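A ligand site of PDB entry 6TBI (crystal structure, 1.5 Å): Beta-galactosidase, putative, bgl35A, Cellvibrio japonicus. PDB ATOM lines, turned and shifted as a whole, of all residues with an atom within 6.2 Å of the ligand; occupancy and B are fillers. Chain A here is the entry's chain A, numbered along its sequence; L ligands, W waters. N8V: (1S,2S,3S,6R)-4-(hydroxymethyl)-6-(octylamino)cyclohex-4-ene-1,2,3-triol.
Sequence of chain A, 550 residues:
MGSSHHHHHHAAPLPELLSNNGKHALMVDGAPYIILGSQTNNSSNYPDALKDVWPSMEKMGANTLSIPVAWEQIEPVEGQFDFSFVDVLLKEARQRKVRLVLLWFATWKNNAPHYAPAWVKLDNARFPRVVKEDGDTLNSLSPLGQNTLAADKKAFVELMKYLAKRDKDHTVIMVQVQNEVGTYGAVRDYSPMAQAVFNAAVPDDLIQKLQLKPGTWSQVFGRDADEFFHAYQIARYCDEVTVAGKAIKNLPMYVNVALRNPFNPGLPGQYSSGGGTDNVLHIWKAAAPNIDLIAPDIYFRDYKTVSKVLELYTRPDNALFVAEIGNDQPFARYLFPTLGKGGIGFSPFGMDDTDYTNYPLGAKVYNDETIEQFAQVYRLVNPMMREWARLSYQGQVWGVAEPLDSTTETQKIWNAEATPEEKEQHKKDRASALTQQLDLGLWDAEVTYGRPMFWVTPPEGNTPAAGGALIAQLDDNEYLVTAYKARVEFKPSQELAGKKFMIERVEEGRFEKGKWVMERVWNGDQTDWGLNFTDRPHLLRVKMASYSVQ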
ATOM      1  N   GLN A  39      19.517 -21.912  28.000  1.00  0.00           N
ATOM      2  CA  GLN A  39      19.515 -20.774  28.943  1.00  0.00           C
ATOM      3  C   GLN A  39      18.836 -21.259  30.240  1.00  0.00           C
ATOM      4  O   GLN A  39      17.840 -21.940  30.230  1.00  0.00           O
ATOM      5  CB  GLN A  39      18.825 -19.518  28.420  1.00  0.00           C
ATOM      6  CG  GLN A  39      18.818 -18.378  29.425  1.00  0.00           C
ATOM      7  CD  GLN A  39      18.356 -17.021  28.968  1.00  0.00           C
ATOM      8  OE1 GLN A  39      17.984 -16.162  29.796  1.00  0.00           O
ATOM      9  NE2 GLN A  39      18.522 -16.723  27.679  1.00  0.00           N
ATOM     10  N   ASN A  41      16.870 -20.770  33.932  1.00  0.00           N
ATOM     11  CA  ASN A  41      15.838 -19.888  34.521  1.00  0.00           C
ATOM     12  C   ASN A  41      16.530 -18.651  35.118  1.00  0.00           C
ATOM     13  O   ASN A  41      17.793 -18.639  35.318  1.00  0.00           O
ATOM     14  CB  ASN A  41      14.958 -20.689  35.472  1.00  0.00           C
ATOM     15  CG  ASN A  41      13.926 -21.506  34.725  1.00  0.00           C
ATOM     16  OD1 ASN A  41      13.035 -20.888  34.098  1.00  0.00           O
ATOM     17  ND2 ASN A  41      13.961 -22.845  34.892  1.00  0.00           N
ATOM     18  N   ASN A  42      15.745 -17.614  35.423  1.00  0.00           N
ATOM     19  CA  ASN A  42      16.179 -16.251  35.806  1.00  0.00           C
ATOM     20  C   ASN A  42      16.838 -16.176  37.210  1.00  0.00           C
ATOM     21  O   ASN A  42      17.462 -15.171  37.480  1.00  0.00           O
ATOM     22  CB  ASN A  42      14.986 -15.324  35.762  1.00  0.00           C
ATOM     23  CG  ASN A  42      14.594 -14.739  34.420  1.00  0.00           C
ATOM     24  OD1 ASN A  42      13.520 -14.101  34.387  1.00  0.00           O
ATOM     25  ND2 ASN A  42      15.358 -15.002  33.334  1.00  0.00           N
ATOM     26  N   PHE A 105      22.399  -8.458  33.349  1.00  0.00           N
ATOM     27  CA  PHE A 105      21.084  -7.989  33.837  1.00  0.00           C
ATOM     28  C   PHE A 105      21.348  -6.749  34.680  1.00  0.00           C
ATOM     29  O   PHE A 105      21.921  -6.904  35.773  1.00  0.00           O
ATOM     30  CB  PHE A 105      20.379  -9.074  34.643  1.00  0.00           C
ATOM     31  CG  PHE A 105      19.735 -10.234  33.924  1.00  0.00           C
ATOM     32  CD1 PHE A 105      19.919 -10.496  32.556  1.00  0.00           C
ATOM     33  CD2 PHE A 105      18.944 -11.118  34.651  1.00  0.00           C
ATOM     34  CE1 PHE A 105      19.294 -11.597  31.981  1.00  0.00           C
ATOM     35  CE2 PHE A 105      18.345 -12.215  34.068  1.00  0.00           C
ATOM     36  CZ  PHE A 105      18.502 -12.444  32.703  1.00  0.00           C
ATOM     37  N   LYS A 109      16.017  -5.335  32.749  1.00  0.00           N
ATOM     38  CA  LYS A 109      15.715  -6.765  32.617  1.00  0.00           C
ATOM     39  C   LYS A 109      14.206  -6.752  32.434  1.00  0.00           C
ATOM     40  O   LYS A 109      13.446  -6.430  33.390  1.00  0.00           O
ATOM     41  CB  LYS A 109      16.250  -7.542  33.833  1.00  0.00           C
ATOM     42  CG  LYS A 109      16.221  -9.055  33.668  1.00  0.00           C
ATOM     43  CD  LYS A 109      14.839  -9.633  33.526  1.00  0.00           C
ATOM     44  CE  LYS A 109      14.833 -11.144  33.464  1.00  0.00           C
ATOM     45  NZ  LYS A 109      13.498 -11.693  33.123  1.00  0.00           N
ATOM     46  N   ASN A 110      13.717  -7.111  31.262  1.00  0.00           N
ATOM     47  CA  ASN A 110      12.292  -7.091  30.939  1.00  0.00           C
ATOM     48  C   ASN A 110      11.733  -5.706  31.316  1.00  0.00           C
ATOM     49  O   ASN A 110      10.704  -5.613  31.999  1.00  0.00           O
ATOM     50  CB  ASN A 110      11.520  -8.220  31.595  1.00  0.00           C
ATOM     51  CG  ASN A 110      11.837  -9.608  31.158  1.00  0.00           C
ATOM     52  OD1 ASN A 110      13.004  -9.877  30.760  1.00  0.00           O
ATOM     53  ND2 ASN A 110      10.876 -10.510  31.391  1.00  0.00           N
ATOM     54  N   ASN A 179      18.809  -7.027  29.293  1.00  0.00           N
ATOM     55  CA  ASN A 179      17.907  -8.097  28.910  1.00  0.00           C
ATOM     56  C   ASN A 179      16.580  -7.452  28.588  1.00  0.00           C
ATOM     57  O   ASN A 179      15.902  -6.923  29.435  1.00  0.00           O
ATOM     58  CB  ASN A 179      17.777  -9.196  30.001  1.00  0.00           C
ATOM     59  CG  ASN A 179      16.916 -10.327  29.520  1.00  0.00           C
ATOM     60  OD1 ASN A 179      17.509 -11.241  28.923  1.00  0.00           O
ATOM     61  ND2 ASN A 179      15.562 -10.286  29.792  1.00  0.00           N
ATOM     62  N   GLU A 180      16.186  -7.530  27.317  1.00  0.00           N
ATOM     63  CA  GLU A 180      14.863  -7.009  26.867  1.00  0.00           C
ATOM     64  C   GLU A 180      14.671  -5.580  27.396  1.00  0.00           C
ATOM     65  O   GLU A 180      13.776  -5.276  28.216  1.00  0.00           O
ATOM     66  CB  GLU A 180      13.756  -7.987  27.218  1.00  0.00           C
ATOM     67  CG  GLU A 180      13.787  -9.222  26.389  1.00  0.00           C
ATOM     68  CD  GLU A 180      12.552 -10.116  26.436  1.00  0.00           C
ATOM     69  OE1 GLU A 180      11.676  -9.867  27.338  1.00  0.00           O
ATOM     70  OE2 GLU A 180      12.468 -11.020  25.584  1.00  0.00           O
ATOM     71  N   TYR A 184       7.266  -0.945  29.274  1.00  0.00           N
ATOM     72  CA  TYR A 184       5.838  -1.283  29.236  1.00  0.00           C
ATOM     73  C   TYR A 184       5.051  -0.160  29.927  1.00  0.00           C
ATOM     74  O   TYR A 184       5.452   0.395  30.968  1.00  0.00           O
ATOM     75  CB  TYR A 184       5.587  -2.628  29.937  1.00  0.00           C
ATOM     76  CG  TYR A 184       6.165  -3.867  29.333  1.00  0.00           C
ATOM     77  CD1 TYR A 184       5.668  -4.342  28.144  1.00  0.00           C
ATOM     78  CD2 TYR A 184       7.191  -4.591  29.926  1.00  0.00           C
ATOM     79  CE1 TYR A 184       6.179  -5.473  27.548  1.00  0.00           C
ATOM     80  CE2 TYR A 184       7.733  -5.722  29.310  1.00  0.00           C
ATOM     81  CZ  TYR A 184       7.196  -6.195  28.137  1.00  0.00           C
ATOM     82  OH  TYR A 184       7.679  -7.273  27.530  1.00  0.00           O
ATOM     83  N   ASN A 256      18.885  -8.448  23.141  1.00  0.00           N
ATOM     84  CA  ASN A 256      17.773  -9.407  22.867  1.00  0.00           C
ATOM     85  C   ASN A 256      16.422  -8.704  22.942  1.00  0.00           C
ATOM     86  O   ASN A 256      16.189  -7.886  23.889  1.00  0.00           O
ATOM     87  CB  ASN A 256      17.854 -10.598  23.834  1.00  0.00           C
ATOM     88  CG  ASN A 256      17.647 -10.252  25.298  1.00  0.00           C
ATOM     89  OD1 ASN A 256      18.161  -9.243  25.749  1.00  0.00           O
ATOM     90  ND2 ASN A 256      17.012 -11.153  26.015  1.00  0.00           N
ATOM     91  N   ALA A 258      12.324  -8.265  23.316  1.00  0.00           N
ATOM     92  CA  ALA A 258      10.920  -8.547  23.638  1.00  0.00           C
ATOM     93  C   ALA A 258      10.116  -8.220  22.371  1.00  0.00           C
ATOM     94  O   ALA A 258       9.751  -7.050  22.158  1.00  0.00           O
ATOM     95  CB  ALA A 258      10.494  -7.775  24.857  1.00  0.00           C
ATOM     96  N   LEU A 259       9.878  -9.286  21.587  1.00  0.00           N
ATOM     97  CA  LEU A 259       9.310  -9.050  20.237  1.00  0.00           C
ATOM     98  C   LEU A 259       7.897  -8.465  20.341  1.00  0.00           C
ATOM     99  O   LEU A 259       7.080  -8.893  21.213  1.00  0.00           O
ATOM    100  CB  LEU A 259       9.222 -10.383  19.505  1.00  0.00           C
ATOM    101  CG  LEU A 259      10.568 -11.039  19.237  1.00  0.00           C
ATOM    102  CD1 LEU A 259      10.298 -12.412  18.622  1.00  0.00           C
ATOM    103  CD2 LEU A 259      11.443 -10.145  18.346  1.00  0.00           C
ATOM    104  N   ASP A 297      13.735 -12.921  20.754  1.00  0.00           N
ATOM    105  CA  ASP A 297      13.363 -13.855  21.850  1.00  0.00           C
ATOM    106  C   ASP A 297      11.974 -14.418  21.473  1.00  0.00           C
ATOM    107  O   ASP A 297      10.979 -13.649  21.554  1.00  0.00           O
ATOM    108  CB  ASP A 297      13.313 -13.119  23.182  1.00  0.00           C
ATOM    109  CG  ASP A 297      14.667 -12.582  23.653  1.00  0.00           C
ATOM    110  OD1 ASP A 297      15.693 -13.159  23.213  1.00  0.00           O
ATOM    111  OD2 ASP A 297      14.671 -11.676  24.563  1.00  0.00           O
ATOM    112  N   TYR A 299       8.661 -16.581  21.517  1.00  0.00           N
ATOM    113  CA  TYR A 299       7.685 -17.365  22.310  1.00  0.00           C
ATOM    114  C   TYR A 299       6.357 -17.499  21.579  1.00  0.00           C
ATOM    115  O   TYR A 299       5.431 -18.089  22.075  1.00  0.00           O
ATOM    116  CB  TYR A 299       7.507 -16.732  23.705  1.00  0.00           C
ATOM    117  CG  TYR A 299       8.762 -16.813  24.520  1.00  0.00           C
ATOM    118  CD1 TYR A 299       9.144 -17.985  25.159  1.00  0.00           C
ATOM    119  CD2 TYR A 299       9.643 -15.751  24.558  1.00  0.00           C
ATOM    120  CE1 TYR A 299      10.313 -18.040  25.902  1.00  0.00           C
ATOM    121  CE2 TYR A 299      10.865 -15.828  25.218  1.00  0.00           C
ATOM    122  CZ  TYR A 299      11.176 -16.964  25.938  1.00  0.00           C
ATOM    123  OH  TYR A 299      12.376 -17.061  26.612  1.00  0.00           O
ATOM    124  N   PHE A 300       6.294 -17.009  20.330  1.00  0.00           N
ATOM    125  CA  PHE A 300       5.118 -17.283  19.480  1.00  0.00           C
ATOM    126  C   PHE A 300       5.159 -18.757  19.097  1.00  0.00           C
ATOM    127  O   PHE A 300       6.234 -19.262  18.735  1.00  0.00           O
ATOM    128  CB  PHE A 300       5.101 -16.438  18.208  1.00  0.00           C
ATOM    129  CG  PHE A 300       5.287 -14.973  18.421  1.00  0.00           C
ATOM    130  CD1 PHE A 300       4.351 -14.224  19.131  1.00  0.00           C
ATOM    131  CD2 PHE A 300       6.400 -14.321  17.936  1.00  0.00           C
ATOM    132  CE1 PHE A 300       4.538 -12.877  19.331  1.00  0.00           C
ATOM    133  CE2 PHE A 300       6.559 -12.959  18.129  1.00  0.00           C
ATOM    134  CZ  PHE A 300       5.664 -12.251  18.852  1.00  0.00           C
ATOM    135  N   ARG A 301       4.070 -19.489  19.224  1.00  0.00           N
ATOM    136  CA  ARG A 301       4.167 -20.969  19.019  1.00  0.00           C
ATOM    137  C   ARG A 301       3.953 -21.378  17.542  1.00  0.00           C
ATOM    138  O   ARG A 301       4.505 -22.506  17.110  1.00  0.00           O
ATOM    139  CB  ARG A 301       3.146 -21.712  19.862  1.00  0.00           C
ATOM    140  CG  ARG A 301       3.579 -21.784  21.326  1.00  0.00           C
ATOM    141  CD  ARG A 301       2.437 -21.789  22.298  1.00  0.00           C
ATOM    142  NE  ARG A 301       3.012 -21.908  23.639  1.00  0.00           N
ATOM    143  CZ  ARG A 301       3.357 -23.084  24.180  1.00  0.00           C
ATOM    144  NH1 ARG A 301       3.183 -24.198  23.505  1.00  0.00           N
ATOM    145  NH2 ARG A 301       3.895 -23.130  25.388  1.00  0.00           N
ATOM    146  N   GLU A 324      16.639 -16.497  22.713  1.00  0.00           N
ATOM    147  CA  GLU A 324      15.673 -17.257  23.524  1.00  0.00           C
ATOM    148  C   GLU A 324      14.616 -17.873  22.657  1.00  0.00           C
ATOM    149  O   GLU A 324      14.173 -17.198  21.716  1.00  0.00           O
ATOM    150  CB  GLU A 324      14.953 -16.383  24.573  1.00  0.00           C
ATOM    151  CG  GLU A 324      15.821 -15.625  25.515  1.00  0.00           C
ATOM    152  CD  GLU A 324      15.065 -14.681  26.454  1.00  0.00           C
ATOM    153  OE1 GLU A 324      13.833 -14.851  26.591  1.00  0.00           O
ATOM    154  OE2 GLU A 324      15.676 -13.645  26.898  1.00  0.00           O
ATOM    155  N   PHE A 349      14.945 -21.509  26.434  1.00  0.00           N
ATOM    156  CA  PHE A 349      14.918 -20.882  27.758  1.00  0.00           C
ATOM    157  C   PHE A 349      14.366 -21.875  28.774  1.00  0.00           C
ATOM    158  O   PHE A 349      13.342 -22.520  28.592  1.00  0.00           O
ATOM    159  CB  PHE A 349      13.986 -19.684  27.740  1.00  0.00           C
ATOM    160  CG  PHE A 349      13.967 -18.927  29.012  1.00  0.00           C
ATOM    161  CD1 PHE A 349      13.170 -19.407  30.043  1.00  0.00           C
ATOM    162  CD2 PHE A 349      14.814 -17.883  29.274  1.00  0.00           C
ATOM    163  CE1 PHE A 349      13.183 -18.776  31.277  1.00  0.00           C
ATOM    164  CE2 PHE A 349      14.827 -17.253  30.508  1.00  0.00           C
ATOM    165  CZ  PHE A 349      14.012 -17.735  31.502  1.00  0.00           C
ATOM    166  N   TYR A 356      10.904 -24.552  38.435  1.00  0.00           N
ATOM    167  CA  TYR A 356      10.116 -23.462  37.817  1.00  0.00           C
ATOM    168  C   TYR A 356       9.702 -23.898  36.430  1.00  0.00           C
ATOM    169  O   TYR A 356      10.546 -24.392  35.731  1.00  0.00           O
ATOM    170  CB  TYR A 356      10.909 -22.160  37.747  1.00  0.00           C
ATOM    171  CG  TYR A 356      10.069 -20.991  37.321  1.00  0.00           C
ATOM    172  CD1 TYR A 356       9.269 -20.281  38.211  1.00  0.00           C
ATOM    173  CD2 TYR A 356      10.099 -20.491  36.015  1.00  0.00           C
ATOM    174  CE1 TYR A 356       8.425 -19.267  37.838  1.00  0.00           C
ATOM    175  CE2 TYR A 356       9.273 -19.453  35.640  1.00  0.00           C
ATOM    176  CZ  TYR A 356       8.402 -18.838  36.515  1.00  0.00           C
ATOM    177  OH  TYR A 356       7.617 -17.741  36.181  1.00  0.00           O
ATOM    178  N   ASN A 358       7.740 -21.909  33.019  1.00  0.00           N
ATOM    179  CA  ASN A 358       7.251 -20.616  32.513  1.00  0.00           C
ATOM    180  C   ASN A 358       6.038 -20.794  31.568  1.00  0.00           C
ATOM    181  O   ASN A 358       5.648 -19.786  30.938  1.00  0.00           O
ATOM    182  CB  ASN A 358       8.371 -19.800  31.892  1.00  0.00           C
ATOM    183  CG  ASN A 358       8.856 -20.290  30.530  1.00  0.00           C
ATOM    184  OD1 ASN A 358       8.491 -21.400  30.119  1.00  0.00           O
ATOM    185  ND2 ASN A 358       9.640 -19.427  29.862  1.00  0.00           N
ATOM    186  N   LEU A 361       4.340 -19.589  28.474  1.00  0.00           N
ATOM    187  CA  LEU A 361       5.398 -19.335  27.465  1.00  0.00           C
ATOM    188  C   LEU A 361       6.041 -20.653  27.006  1.00  0.00           C
ATOM    189  O   LEU A 361       6.195 -20.864  25.839  1.00  0.00           O
ATOM    190  CB  LEU A 361       6.446 -18.390  28.037  1.00  0.00           C
ATOM    191  CG  LEU A 361       6.036 -16.925  28.161  1.00  0.00           C
ATOM    192  CD1 LEU A 361       7.283 -16.053  28.387  1.00  0.00           C
ATOM    193  CD2 LEU A 361       5.240 -16.387  26.988  1.00  0.00           C
HETATM  194  O2  N8V L   1      13.962 -12.174  28.327  1.00  0.00           O
HETATM  195  C2  N8V L   1      12.850 -12.726  29.069  1.00  0.00           C
HETATM  196  C3  N8V L   1      13.385 -13.861  29.915  1.00  0.00           C
HETATM  197  O3  N8V L   1      14.358 -13.328  30.830  1.00  0.00           O
HETATM  198  C4  N8V L   1      12.242 -14.512  30.650  1.00  0.00           C
HETATM  199  O4  N8V L   1      11.591 -13.502  31.405  1.00  0.00           O
HETATM  200  C1  N8V L   1      11.715 -13.200  28.147  1.00  0.00           C
HETATM  201  C7  N8V L   1      11.098 -14.486  28.463  1.00  0.00           C
HETATM  202  C5  N8V L   1      11.376 -15.140  29.616  1.00  0.00           C
HETATM  203  C6  N8V L   1      10.947 -16.601  29.688  1.00  0.00           C
HETATM  204  O6  N8V L   1      10.202 -16.785  30.908  1.00  0.00           O
HETATM  205  N8  N8V L   1      10.619 -12.186  28.027  1.00  0.00           N
HETATM  206  C9  N8V L   1       9.549 -12.430  27.101  1.00  0.00           C
HETATM  207  C10 N8V L   1       8.510 -11.265  27.081  1.00  0.00           C
HETATM  208  C11 N8V L   1       7.386 -11.419  26.072  1.00  0.00           C
HETATM  209  C12 N8V L   1       6.602 -12.658  26.257  1.00  0.00           C
HETATM  210  C13 N8V L   1       5.197 -12.656  25.671  1.00  0.00           C
HETATM  211  C14 N8V L   1       5.158 -13.734  24.573  1.00  0.00           C
HETATM  212  C15 N8V L   1       3.800 -13.995  23.971  1.00  0.00           C
HETATM  213  C16 N8V L   1       3.964 -14.887  22.782  1.00  0.00           C
HETATM  214  O   HOH W   1       8.923 -12.690  30.255  1.00  0.00           O
HETATM  215  O   HOH W   2      16.837 -13.763  29.930  1.00  0.00           O
HETATM  216  O   HOH W   3       6.357  -8.352  25.431  1.00  0.00           O
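A nitrogen (N8) of the ligand lies within salt-bridge range of the side-chain carboxylate (OE1) of Glu 180. The side-chain carboxylate (OE2) of Glu 324 lies within hydrogen-bond range of an oxygen (O2) of the ligand (2.7 Å). An oxygen (O2) of the ligand sits at hydrogen-bond distance from the side-chain amide nitrogen (ND2) of Asn 179 (2.9 Å). ND2 of Asn 358 sits at hydrogen-bond distance from O6 of the ligand (2.9 Å). O3 of the ligand lies within hydrogen-bond range of NZ of Lys 109. O4 of the ligand lies within hydrogen-bond range of ND2 of Asn 110, 3.1 Å away. The side-chain amide nitrogen of Asn 42 sits at hydrogen-bond distance from an oxygen (O3) of the ligand (3.2 Å).
N of Glu 180 sits at hydrogen-bond distance from OD1 of Asn 256 (3.0 Å). OH of Tyr 299 lies within hydrogen-bond range of OE1 of Glu 324, at 2.6 Å. The side-chain carboxylate of Glu 324 lies within hydrogen-bond range of the side-chain amide nitrogen of Asn 256 (3.0 Å). OD1 of Asn 110 is in hydrogen-bond range of ND2 of Asn 179, 2.8 Å away. ND2 of Asn 256 sits at hydrogen-bond distance from OD1 of Asn 179, 3.0 Å away. OD1 of Asn 110 sits at hydrogen-bond distance from NZ of Lys 109, 3.0 Å away. NZ of Lys 109 is in hydrogen-bond range of OD1 of Asn 42, 2.7 Å away. O of Leu 361 sits at hydrogen-bond distance from NH2 of Arg 301.
Merely in contact with the ligand: Asn 256, Asp 297, Tyr 299, Phe 300, Phe 349 and Leu 361. Hydrophobic or aromatic side chains that line the ligand: Tyr 299, Phe 300, Phe 349 and Leu 361. Of the 21 residues printed, 13 come within 4 Å of the ligand. The nearest printed residue that does not touch the ligand is Tyr 184 (4.1 Å).
Water W1 lies within hydrogen-bond range of N8 of the ligand (2.8 Å) and ND2 of Asn 110 (3.1 Å).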
